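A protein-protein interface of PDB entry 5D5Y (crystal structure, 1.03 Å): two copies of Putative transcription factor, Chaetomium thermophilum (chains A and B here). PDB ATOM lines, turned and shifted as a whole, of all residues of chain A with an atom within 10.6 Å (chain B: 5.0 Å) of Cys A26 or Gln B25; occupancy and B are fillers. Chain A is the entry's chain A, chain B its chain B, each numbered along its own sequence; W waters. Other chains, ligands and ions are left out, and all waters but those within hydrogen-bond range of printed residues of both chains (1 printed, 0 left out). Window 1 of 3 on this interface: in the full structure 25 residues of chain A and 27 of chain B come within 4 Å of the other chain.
Of the printed residues of chain B, Leu A22 touches Leu B22 (3.6 Å).
Printed residues of chain B within 4 Å of Gln A23: Ala B21, Leu B22 and Gln B25.
Cys A26 touches just these residues of chain B: Gln B25 (3.8 Å) and Cys B26 (2.1 Å).
Of the printed residues of chain B, Leu A29 touches Leu B29.
Printed residues of chain B within 4 Å of Glu A30: Glu B28 (3.7 Å) and Leu B29 (3.7 Å).
Asn A33 touches none of the printed residues of chain B.
Ala B21 touches one residue of chain A.
Printed residues of chain A within 4 Å of Leu B22: Leu A19 (3.8 Å), Leu A22 (3.6 Å) and Gln A23 (3.4 Å).
Gln B25 touches just these residues of chain A: Gln A23 (3.4 Å), Cys A26 (3.8 Å) and Tyr A27 (3.5 Å).
Cys B26 touches just one residue of chain A: Cys A26 (2.1 Å).
Tyr B27 touches none of the printed residues of chain A.
Of chain A, only Glu A30 (3.7 Å) comes within 4 Å of Glu B28.
Leu B29 touches just these residues of chain A: Leu A29 and Glu A30.
The nearest residue of chain A that does not touch Gln B25 is Glu A30 (4.4 Å).
The nearest printed residue of chain B that does not touch Leu A22 is Cys B26 (4.6 Å).
Leu A19 touches Leu B22 (CD2 to CD2, 3.8 Å).
Leu A22 touches Leu B22 (C to CD1, 3.6 Å).
Gln A23 touches Ala B21 (OE1 to CB, 3.6 Å).
Gln A23 touches Leu B22.
Gln A23 touches Gln B25 (O to CG, 3.4 Å).
CG of Gln B25 touches CB of Cys A26, at 3.8 Å.
Gln B25 touches Tyr A27.
C of Leu A29 touches CD1 of Leu B29 (3.8 Å).
Glu B28 touches Glu A30 (O to CG, 3.7 Å).
Glu A30 touches Leu B29.
The guanidinium group (NH2) of Arg A34 lies within salt-bridge range of the side-chain carboxylate (OE1) of Glu A30 (2.8 Å).
Water W1 lies within hydrogen-bond range of NE2 of Gln B25 (2.7 Å) and NE2 of Gln A23 (2.8 Å).
Gln A23 touches Leu B22, but with the chains exchanged Leu A22 does not touch Gln B23 (7.9 Å).
Gln A23 touches Gln B25, but with the chains exchanged Gln A25 does not touch Gln B23 (10.7 Å).
Cys A26 touches Gln B25, but with the chains exchanged Gln A25 does not touch Cys B26 (6.2 Å).
Leu B29 touches its own counterpart, Leu A29.
Positions printed for both chains: 21, 22, 23, 24, 25, 26, 27, 28 and 29.
Of the 9 printed residues of chain B, 6 touch a printed residue of chain A.
Hydrophobic or aromatic side chains of chain A within 4 Å of the printed part of chain B: Leu A19, Leu A22, Tyr A27 and Leu A29.
Along chain A the printed residues that touch a printed residue of chain B span positions 19 to 30.
Among the printed residues, 11 pairs touch across the chains.
Among the printed residues, no Asp or Glu carboxylate lies within 4 Å of a Lys or Arg side-chain nitrogen of the other chain.
The side-chain sulfur (SG) of Cys B26 is disulfide-bonded to the side-chain sulfur (SG) of Cys A26 (2.1 Å).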
ATOM      1  N   GLN A  18     -26.032  20.486  -1.059  1.00  0.00           N
ATOM      2  CA  GLN A  18     -27.266  20.688  -0.275  1.00  0.00           C
ATOM      3  C   GLN A  18     -27.687  19.446   0.479  1.00  0.00           C
ATOM      4  O   GLN A  18     -28.155  19.511   1.656  1.00  0.00           O
ATOM      5  CB  GLN A  18     -28.361  21.123  -1.246  1.00  0.00           C
ATOM      6  CG  GLN A  18     -28.170  22.486  -1.778  1.00  0.00           C
ATOM      7  CD  GLN A  18     -29.276  22.827  -2.758  1.00  0.00           C
ATOM      8  OE1 GLN A  18     -29.433  22.196  -3.790  1.00  0.00           O
ATOM      9  NE2 GLN A  18     -30.102  23.755  -2.376  1.00  0.00           N
ATOM     10  N   LEU A  19     -27.495  18.274  -0.109  1.00  0.00           N
ATOM     11  CA  LEU A  19     -27.699  16.997   0.600  1.00  0.00           C
ATOM     12  C   LEU A  19     -26.728  16.858   1.762  1.00  0.00           C
ATOM     13  O   LEU A  19     -27.114  16.419   2.844  1.00  0.00           O
ATOM     14  CB  LEU A  19     -27.530  15.837  -0.341  1.00  0.00           C
ATOM     15  CG  LEU A  19     -28.586  15.766  -1.440  1.00  0.00           C
ATOM     16  CD1 LEU A  19     -28.205  14.636  -2.372  1.00  0.00           C
ATOM     17  CD2 LEU A  19     -29.962  15.570  -0.868  1.00  0.00           C
ATOM     18  N   GLN A  20     -25.486  17.263   1.570  1.00  0.00           N
ATOM     19  CA  GLN A  20     -24.502  17.215   2.643  1.00  0.00           C
ATOM     20  C   GLN A  20     -24.924  18.127   3.806  1.00  0.00           C
ATOM     21  O   GLN A  20     -24.756  17.780   4.995  1.00  0.00           O
ATOM     22  CB  GLN A  20     -23.164  17.693   2.129  1.00  0.00           C
ATOM     23  CG  GLN A  20     -21.980  17.246   2.933  1.00  0.00           C
ATOM     24  CD  GLN A  20     -20.712  17.400   2.115  1.00  0.00           C
ATOM     25  OE1 GLN A  20     -20.753  17.513   0.860  1.00  0.00           O
ATOM     26  NE2 GLN A  20     -19.579  17.392   2.801  1.00  0.00           N
ATOM     27  N   ALA A  21     -25.440  19.308   3.511  1.00  0.00           N
ATOM     28  CA  ALA A  21     -25.904  20.227   4.559  1.00  0.00           C
ATOM     29  C   ALA A  21     -27.093  19.620   5.333  1.00  0.00           C
ATOM     30  O   ALA A  21     -27.173  19.745   6.564  1.00  0.00           O
ATOM     31  CB  ALA A  21     -26.286  21.569   3.955  1.00  0.00           C
ATOM     32  N   LEU A  22     -28.006  18.978   4.635  1.00  0.00           N
ATOM     33  CA  LEU A  22     -29.093  18.264   5.324  1.00  0.00           C
ATOM     34  C   LEU A  22     -28.583  17.127   6.184  1.00  0.00           C
ATOM     35  O   LEU A  22     -29.101  16.889   7.301  1.00  0.00           O
ATOM     36  CB  LEU A  22     -30.102  17.731   4.306  1.00  0.00           C
ATOM     37  CG  LEU A  22     -31.049  18.784   3.728  1.00  0.00           C
ATOM     38  CD1 LEU A  22     -31.570  18.362   2.390  1.00  0.00           C
ATOM     39  CD2 LEU A  22     -32.208  19.036   4.689  1.00  0.00           C
ATOM     40  N   GLN A  23     -27.562  16.419   5.700  1.00  0.00           N
ATOM     41  CA  GLN A  23     -26.987  15.340   6.467  1.00  0.00           C
ATOM     42  C   GLN A  23     -26.369  15.888   7.774  1.00  0.00           C
ATOM     43  O   GLN A  23     -26.540  15.330   8.849  1.00  0.00           O
ATOM     44  CB  GLN A  23     -25.940  14.621   5.628  1.00  0.00           C
ATOM     45  CG  GLN A  23     -25.356  13.415   6.345  1.00  0.00           C
ATOM     46  CD  GLN A  23     -24.353  12.701   5.498  1.00  0.00           C
ATOM     47  OE1 GLN A  23     -24.329  12.840   4.300  1.00  0.00           O
ATOM     48  NE2 GLN A  23     -23.479  11.993   6.143  1.00  0.00           N
ATOM     49  N   GLN A  24     -25.692  17.015   7.667  1.00  0.00           N
ATOM     50  CA  GLN A  24     -25.116  17.655   8.828  1.00  0.00           C
ATOM     51  C   GLN A  24     -26.215  18.095   9.809  1.00  0.00           C
ATOM     52  O   GLN A  24     -26.023  18.013  11.039  1.00  0.00           O
ATOM     53  CB  GLN A  24     -24.263  18.844   8.365  1.00  0.00           C
ATOM     54  CG  GLN A  24     -23.682  19.595   9.508  1.00  0.00           C
ATOM     55  CD  GLN A  24     -22.609  18.845  10.245  1.00  0.00           C
ATOM     56  OE1 GLN A  24     -22.013  17.912   9.734  1.00  0.00           O
ATOM     57  NE2 GLN A  24     -22.328  19.271  11.504  1.00  0.00           N
ATOM     58  N   GLN A  25     -27.327  18.593   9.314  1.00  0.00           N
ATOM     59  CA  GLN A  25     -28.444  18.973  10.173  1.00  0.00           C
ATOM     60  C   GLN A  25     -28.988  17.749  10.918  1.00  0.00           C
ATOM     61  O   GLN A  25     -29.193  17.831  12.150  1.00  0.00           O
ATOM     62  CB  GLN A  25     -29.526  19.627   9.311  1.00  0.00           C
ATOM     63  CG  GLN A  25     -30.692  20.182  10.069  1.00  0.00           C
ATOM     64  CD  GLN A  25     -31.595  20.999   9.171  1.00  0.00           C
ATOM     65  OE1 GLN A  25     -32.084  20.511   8.134  1.00  0.00           O
ATOM     66  NE2 GLN A  25     -31.776  22.225   9.504  1.00  0.00           N
ATOM     67  N   CYS A  26     -29.195  16.632  10.243  1.00  0.00           N
ATOM     68  CA  CYS A  26     -29.626  15.435  10.956  1.00  0.00           C
ATOM     69  C   CYS A  26     -28.609  14.972  11.966  1.00  0.00           C
ATOM     70  O   CYS A  26     -28.984  14.510  13.063  1.00  0.00           O
ATOM     71  CB  CYS A  26     -29.984  14.323   9.972  1.00  0.00           C
ATOM     72  SG  CYS A  26     -31.668  14.507   9.313  1.00  0.00           S
ATOM     73  N   TYR A  27     -27.321  15.055  11.622  1.00  0.00           N
ATOM     74  CA  TYR A  27     -26.238  14.708  12.544  1.00  0.00           C
ATOM     75  C   TYR A  27     -26.292  15.556  13.809  1.00  0.00           C
ATOM     76  O   TYR A  27     -26.214  15.023  14.933  1.00  0.00           O
ATOM     77  CB  TYR A  27     -24.904  14.910  11.804  1.00  0.00           C
ATOM     78  CG  TYR A  27     -23.703  14.716  12.684  1.00  0.00           C
ATOM     79  CD1 TYR A  27     -23.186  13.457  12.939  1.00  0.00           C
ATOM     80  CD2 TYR A  27     -23.046  15.772  13.273  1.00  0.00           C
ATOM     81  CE1 TYR A  27     -22.086  13.244  13.707  1.00  0.00           C
ATOM     82  CE2 TYR A  27     -21.930  15.593  14.082  1.00  0.00           C
ATOM     83  CZ  TYR A  27     -21.424  14.347  14.249  1.00  0.00           C
ATOM     84  OH  TYR A  27     -20.320  14.044  15.057  1.00  0.00           O
ATOM     85  N   GLU A  28     -26.423  16.861  13.648  1.00  0.00           N
ATOM     86  CA  GLU A  28     -26.425  17.771  14.791  1.00  0.00           C
ATOM     87  C   GLU A  28     -27.656  17.528  15.665  1.00  0.00           C
ATOM     88  O   GLU A  28     -27.559  17.522  16.904  1.00  0.00           O
ATOM     89  CB  GLU A  28     -26.389  19.210  14.343  1.00  0.00           C
ATOM     90  CG  GLU A  28     -25.020  19.588  13.772  1.00  0.00           C
ATOM     91  CD  GLU A  28     -24.937  20.986  13.274  1.00  0.00           C
ATOM     92  OE1 GLU A  28     -25.879  21.810  13.543  1.00  0.00           O
ATOM     93  OE2 GLU A  28     -23.903  21.358  12.700  1.00  0.00           O
ATOM     94  N   LEU A  29     -28.816  17.387  15.036  1.00  0.00           N
ATOM     95  CA  LEU A  29     -30.048  17.145  15.790  1.00  0.00           C
ATOM     96  C   LEU A  29     -29.982  15.831  16.551  1.00  0.00           C
ATOM     97  O   LEU A  29     -30.440  15.732  17.706  1.00  0.00           O
ATOM     98  CB  LEU A  29     -31.259  17.146  14.875  1.00  0.00           C
ATOM     99  CG  LEU A  29     -31.662  18.526  14.316  1.00  0.00           C
ATOM    100  CD1 LEU A  29     -32.622  18.356  13.162  1.00  0.00           C
ATOM    101  CD2 LEU A  29     -32.216  19.410  15.411  1.00  0.00           C
ATOM    102  N   GLU A  30     -29.395  14.792  15.930  1.00  0.00           N
ATOM    103  CA  GLU A  30     -29.290  13.506  16.604  1.00  0.00           C
ATOM    104  C   GLU A  30     -28.410  13.641  17.842  1.00  0.00           C
ATOM    105  O   GLU A  30     -28.753  13.115  18.917  1.00  0.00           O
ATOM    106  CB  GLU A  30     -28.751  12.454  15.666  1.00  0.00           C
ATOM    107  CG  GLU A  30     -28.810  11.058  16.266  1.00  0.00           C
ATOM    108  CD  GLU A  30     -27.758  10.674  17.297  1.00  0.00           C
ATOM    109  OE1 GLU A  30     -26.652  11.227  17.258  1.00  0.00           O
ATOM    110  OE2 GLU A  30     -28.070   9.789  18.147  1.00  0.00           O
ATOM    111  N   LYS A  31     -27.280  14.329  17.731  1.00  0.00           N
ATOM    112  CA  LYS A  31     -26.385  14.471  18.871  1.00  0.00           C
ATOM    113  C   LYS A  31     -27.063  15.303  19.964  1.00  0.00           C
ATOM    114  O   LYS A  31     -26.994  14.937  21.165  1.00  0.00           O
ATOM    115  CB  LYS A  31     -25.069  15.070  18.449  1.00  0.00           C
ATOM    116  CG  LYS A  31     -24.143  15.077  19.611  1.00  0.00           C
ATOM    117  CD  LYS A  31     -22.802  15.613  19.361  1.00  0.00           C
ATOM    118  CE  LYS A  31     -21.919  15.492  20.613  1.00  0.00           C
ATOM    119  NZ  LYS A  31     -20.672  16.235  20.486  1.00  0.00           N
ATOM    120  N   THR A  32     -27.689  16.383  19.595  1.00  0.00           N
ATOM    121  CA  THR A  32     -28.405  17.207  20.558  1.00  0.00           C
ATOM    122  C   THR A  32     -29.464  16.399  21.299  1.00  0.00           C
ATOM    123  O   THR A  32     -29.561  16.487  22.540  1.00  0.00           O
ATOM    124  CB  THR A  32     -29.048  18.385  19.836  1.00  0.00           C
ATOM    125  OG1 THR A  32     -28.007  19.216  19.314  1.00  0.00           O
ATOM    126  CG2 THR A  32     -30.007  19.179  20.698  1.00  0.00           C
ATOM    127  N   ASN A  33     -30.227  15.603  20.577  1.00  0.00           N
ATOM    128  CA  ASN A  33     -31.318  14.887  21.215  1.00  0.00           C
ATOM    129  C   ASN A  33     -30.844  13.710  22.010  1.00  0.00           C
ATOM    130  O   ASN A  33     -31.465  13.364  23.034  1.00  0.00           O
ATOM    131  CB  ASN A  33     -32.418  14.590  20.213  1.00  0.00           C
ATOM    132  CG  ASN A  33     -33.191  15.858  19.861  1.00  0.00           C
ATOM    133  OD1 ASN A  33     -32.829  16.939  20.296  1.00  0.00           O
ATOM    134  ND2 ASN A  33     -34.245  15.721  19.067  1.00  0.00           N
ATOM    135  N   ARG A  34     -29.724  13.097  21.625  1.00  0.00           N
ATOM    136  CA  ARG A  34     -29.131  12.050  22.428  1.00  0.00           C
ATOM    137  C   ARG A  34     -28.617  12.599  23.757  1.00  0.00           C
ATOM    138  O   ARG A  34     -28.812  11.993  24.834  1.00  0.00           O
ATOM    139  CB  ARG A  34     -27.988  11.385  21.622  1.00  0.00           C
ATOM    140  CG  ARG A  34     -27.284  10.300  22.379  1.00  0.00           C
ATOM    141  CD  ARG A  34     -26.588   9.331  21.396  1.00  0.00           C
ATOM    142  NE  ARG A  34     -25.993   9.994  20.220  1.00  0.00           N
ATOM    143  CZ  ARG A  34     -24.811  10.564  20.138  1.00  0.00           C
ATOM    144  NH1 ARG A  34     -23.969  10.678  21.137  1.00  0.00           N
ATOM    145  NH2 ARG A  34     -24.460  10.964  18.931  1.00  0.00           N
ATOM    146  N   ALA B  21     -26.367   8.335   2.299  1.00  0.00           N
ATOM    147  CA  ALA B  21     -25.768   8.734   3.574  1.00  0.00           C
ATOM    148  C   ALA B  21     -26.708   9.670   4.348  1.00  0.00           C
ATOM    149  O   ALA B  21     -26.781   9.600   5.592  1.00  0.00           O
ATOM    150  CB  ALA B  21     -24.451   9.424   3.341  1.00  0.00           C
ATOM    151  N   LEU B  22     -27.420  10.520   3.669  1.00  0.00           N
ATOM    152  CA  LEU B  22     -28.427  11.378   4.292  1.00  0.00           C
ATOM    153  C   LEU B  22     -29.558  10.558   4.887  1.00  0.00           C
ATOM    154  O   LEU B  22     -29.942  10.764   6.059  1.00  0.00           O
ATOM    155  CB  LEU B  22     -28.954  12.386   3.239  1.00  0.00           C
ATOM    156  CG  LEU B  22     -30.183  13.183   3.693  1.00  0.00           C
ATOM    157  CD1 LEU B  22     -29.889  14.002   4.941  1.00  0.00           C
ATOM    158  CD2 LEU B  22     -30.593  14.095   2.525  1.00  0.00           C
ATOM    159  N   GLN B  23     -30.056   9.587   4.141  1.00  0.00           N
ATOM    160  CA  GLN B  23     -31.078   8.707   4.656  1.00  0.00           C
ATOM    161  C   GLN B  23     -30.659   7.996   5.918  1.00  0.00           C
ATOM    162  O   GLN B  23     -31.397   7.937   6.900  1.00  0.00           O
ATOM    163  CB  GLN B  23     -31.521   7.671   3.625  1.00  0.00           C
ATOM    164  CG  GLN B  23     -32.185   8.234   2.443  1.00  0.00           C
ATOM    165  CD  GLN B  23     -32.312   7.190   1.279  1.00  0.00           C
ATOM    166  OE1 GLN B  23     -33.383   7.043   0.704  1.00  0.00           O
ATOM    167  NE2 GLN B  23     -31.240   6.480   0.905  1.00  0.00           N
ATOM    168  N   GLN B  24     -29.447   7.490   5.916  1.00  0.00           N
ATOM    169  CA  GLN B  24     -28.928   6.773   7.068  1.00  0.00           C
ATOM    170  C   GLN B  24     -28.783   7.692   8.291  1.00  0.00           C
ATOM    171  O   GLN B  24     -29.131   7.340   9.418  1.00  0.00           O
ATOM    172  CB  GLN B  24     -27.574   6.160   6.746  1.00  0.00           C
ATOM    173  CG  GLN B  24     -27.611   5.054   5.727  1.00  0.00           C
ATOM    174  CD  GLN B  24     -27.973   3.737   6.359  1.00  0.00           C
ATOM    175  OE1 GLN B  24     -28.326   3.661   7.563  1.00  0.00           O
ATOM    176  NE2 GLN B  24     -27.907   2.674   5.586  1.00  0.00           N
ATOM    177  N   GLN B  25     -28.286   8.889   8.074  1.00  0.00           N
ATOM    178  CA  GLN B  25     -28.130   9.848   9.181  1.00  0.00           C
ATOM    179  C   GLN B  25     -29.472  10.265   9.775  1.00  0.00           C
ATOM    180  O   GLN B  25     -29.614  10.389  10.995  1.00  0.00           O
ATOM    181  CB  GLN B  25     -27.325  11.034   8.692  1.00  0.00           C
ATOM    182  CG  GLN B  25     -26.989  12.048   9.799  1.00  0.00           C
ATOM    183  CD  GLN B  25     -26.176  11.462  10.916  1.00  0.00           C
ATOM    184  OE1 GLN B  25     -26.745  11.095  12.004  1.00  0.00           O
ATOM    185  NE2 GLN B  25     -24.908  11.355  10.749  1.00  0.00           N
ATOM    186  N   CYS B  26     -30.456  10.562   8.934  1.00  0.00           N
ATOM    187  CA  CYS B  26     -31.752  10.970   9.437  1.00  0.00           C
ATOM    188  C   CYS B  26     -32.487   9.790  10.099  1.00  0.00           C
ATOM    189  O   CYS B  26     -33.261   9.998  11.042  1.00  0.00           O
ATOM    190  CB  CYS B  26     -32.557  11.723   8.391  1.00  0.00           C
ATOM    191  SG  CYS B  26     -31.757  13.200   7.733  1.00  0.00           S
ATOM    192  N   TYR B  27     -32.243   8.571   9.640  1.00  0.00           N
ATOM    193  CA  TYR B  27     -32.733   7.384  10.358  1.00  0.00           C
ATOM    194  C   TYR B  27     -32.183   7.341  11.795  1.00  0.00           C
ATOM    195  O   TYR B  27     -32.943   7.014  12.729  1.00  0.00           O
ATOM    196  CB  TYR B  27     -32.319   6.116   9.602  1.00  0.00           C
ATOM    197  CG  TYR B  27     -32.451   4.779  10.402  1.00  0.00           C
ATOM    198  CD1 TYR B  27     -33.616   4.198  10.596  1.00  0.00           C
ATOM    199  CD2 TYR B  27     -31.361   4.201  11.028  1.00  0.00           C
ATOM    200  CE1 TYR B  27     -33.766   2.996  11.303  1.00  0.00           C
ATOM    201  CE2 TYR B  27     -31.452   3.053  11.759  1.00  0.00           C
ATOM    202  CZ  TYR B  27     -32.655   2.438  11.898  1.00  0.00           C
ATOM    203  OH  TYR B  27     -32.683   1.313  12.650  1.00  0.00           O
ATOM    204  N   GLU B  28     -30.924   7.650  11.991  1.00  0.00           N
ATOM    205  CA  GLU B  28     -30.365   7.661  13.337  1.00  0.00           C
ATOM    206  C   GLU B  28     -31.062   8.734  14.184  1.00  0.00           C
ATOM    207  O   GLU B  28     -31.303   8.504  15.389  1.00  0.00           O
ATOM    208  CB  GLU B  28     -28.864   7.885  13.344  1.00  0.00           C
ATOM    209  CG  GLU B  28     -28.064   6.739  12.709  1.00  0.00           C
ATOM    210  CD  GLU B  28     -28.281   5.371  13.310  1.00  0.00           C
ATOM    211  OE1 GLU B  28     -28.600   5.246  14.463  1.00  0.00           O
ATOM    212  OE2 GLU B  28     -28.140   4.389  12.589  1.00  0.00           O
ATOM    213  N   LEU B  29     -31.341   9.885  13.609  1.00  0.00           N
ATOM    214  CA  LEU B  29     -32.106  10.912  14.316  1.00  0.00           C
ATOM    215  C   LEU B  29     -33.461  10.376  14.728  1.00  0.00           C
ATOM    216  O   LEU B  29     -33.883  10.539  15.882  1.00  0.00           O
ATOM    217  CB  LEU B  29     -32.246  12.168  13.456  1.00  0.00           C
ATOM    218  CG  LEU B  29     -33.223  13.212  14.007  1.00  0.00           C
ATOM    219  CD1 LEU B  29     -32.852  13.708  15.388  1.00  0.00           C
ATOM    220  CD2 LEU B  29     -33.318  14.361  13.012  1.00  0.00           C
HETATM  221  O   HOH W   1     -23.246  12.516   8.903  1.00  0.00           O
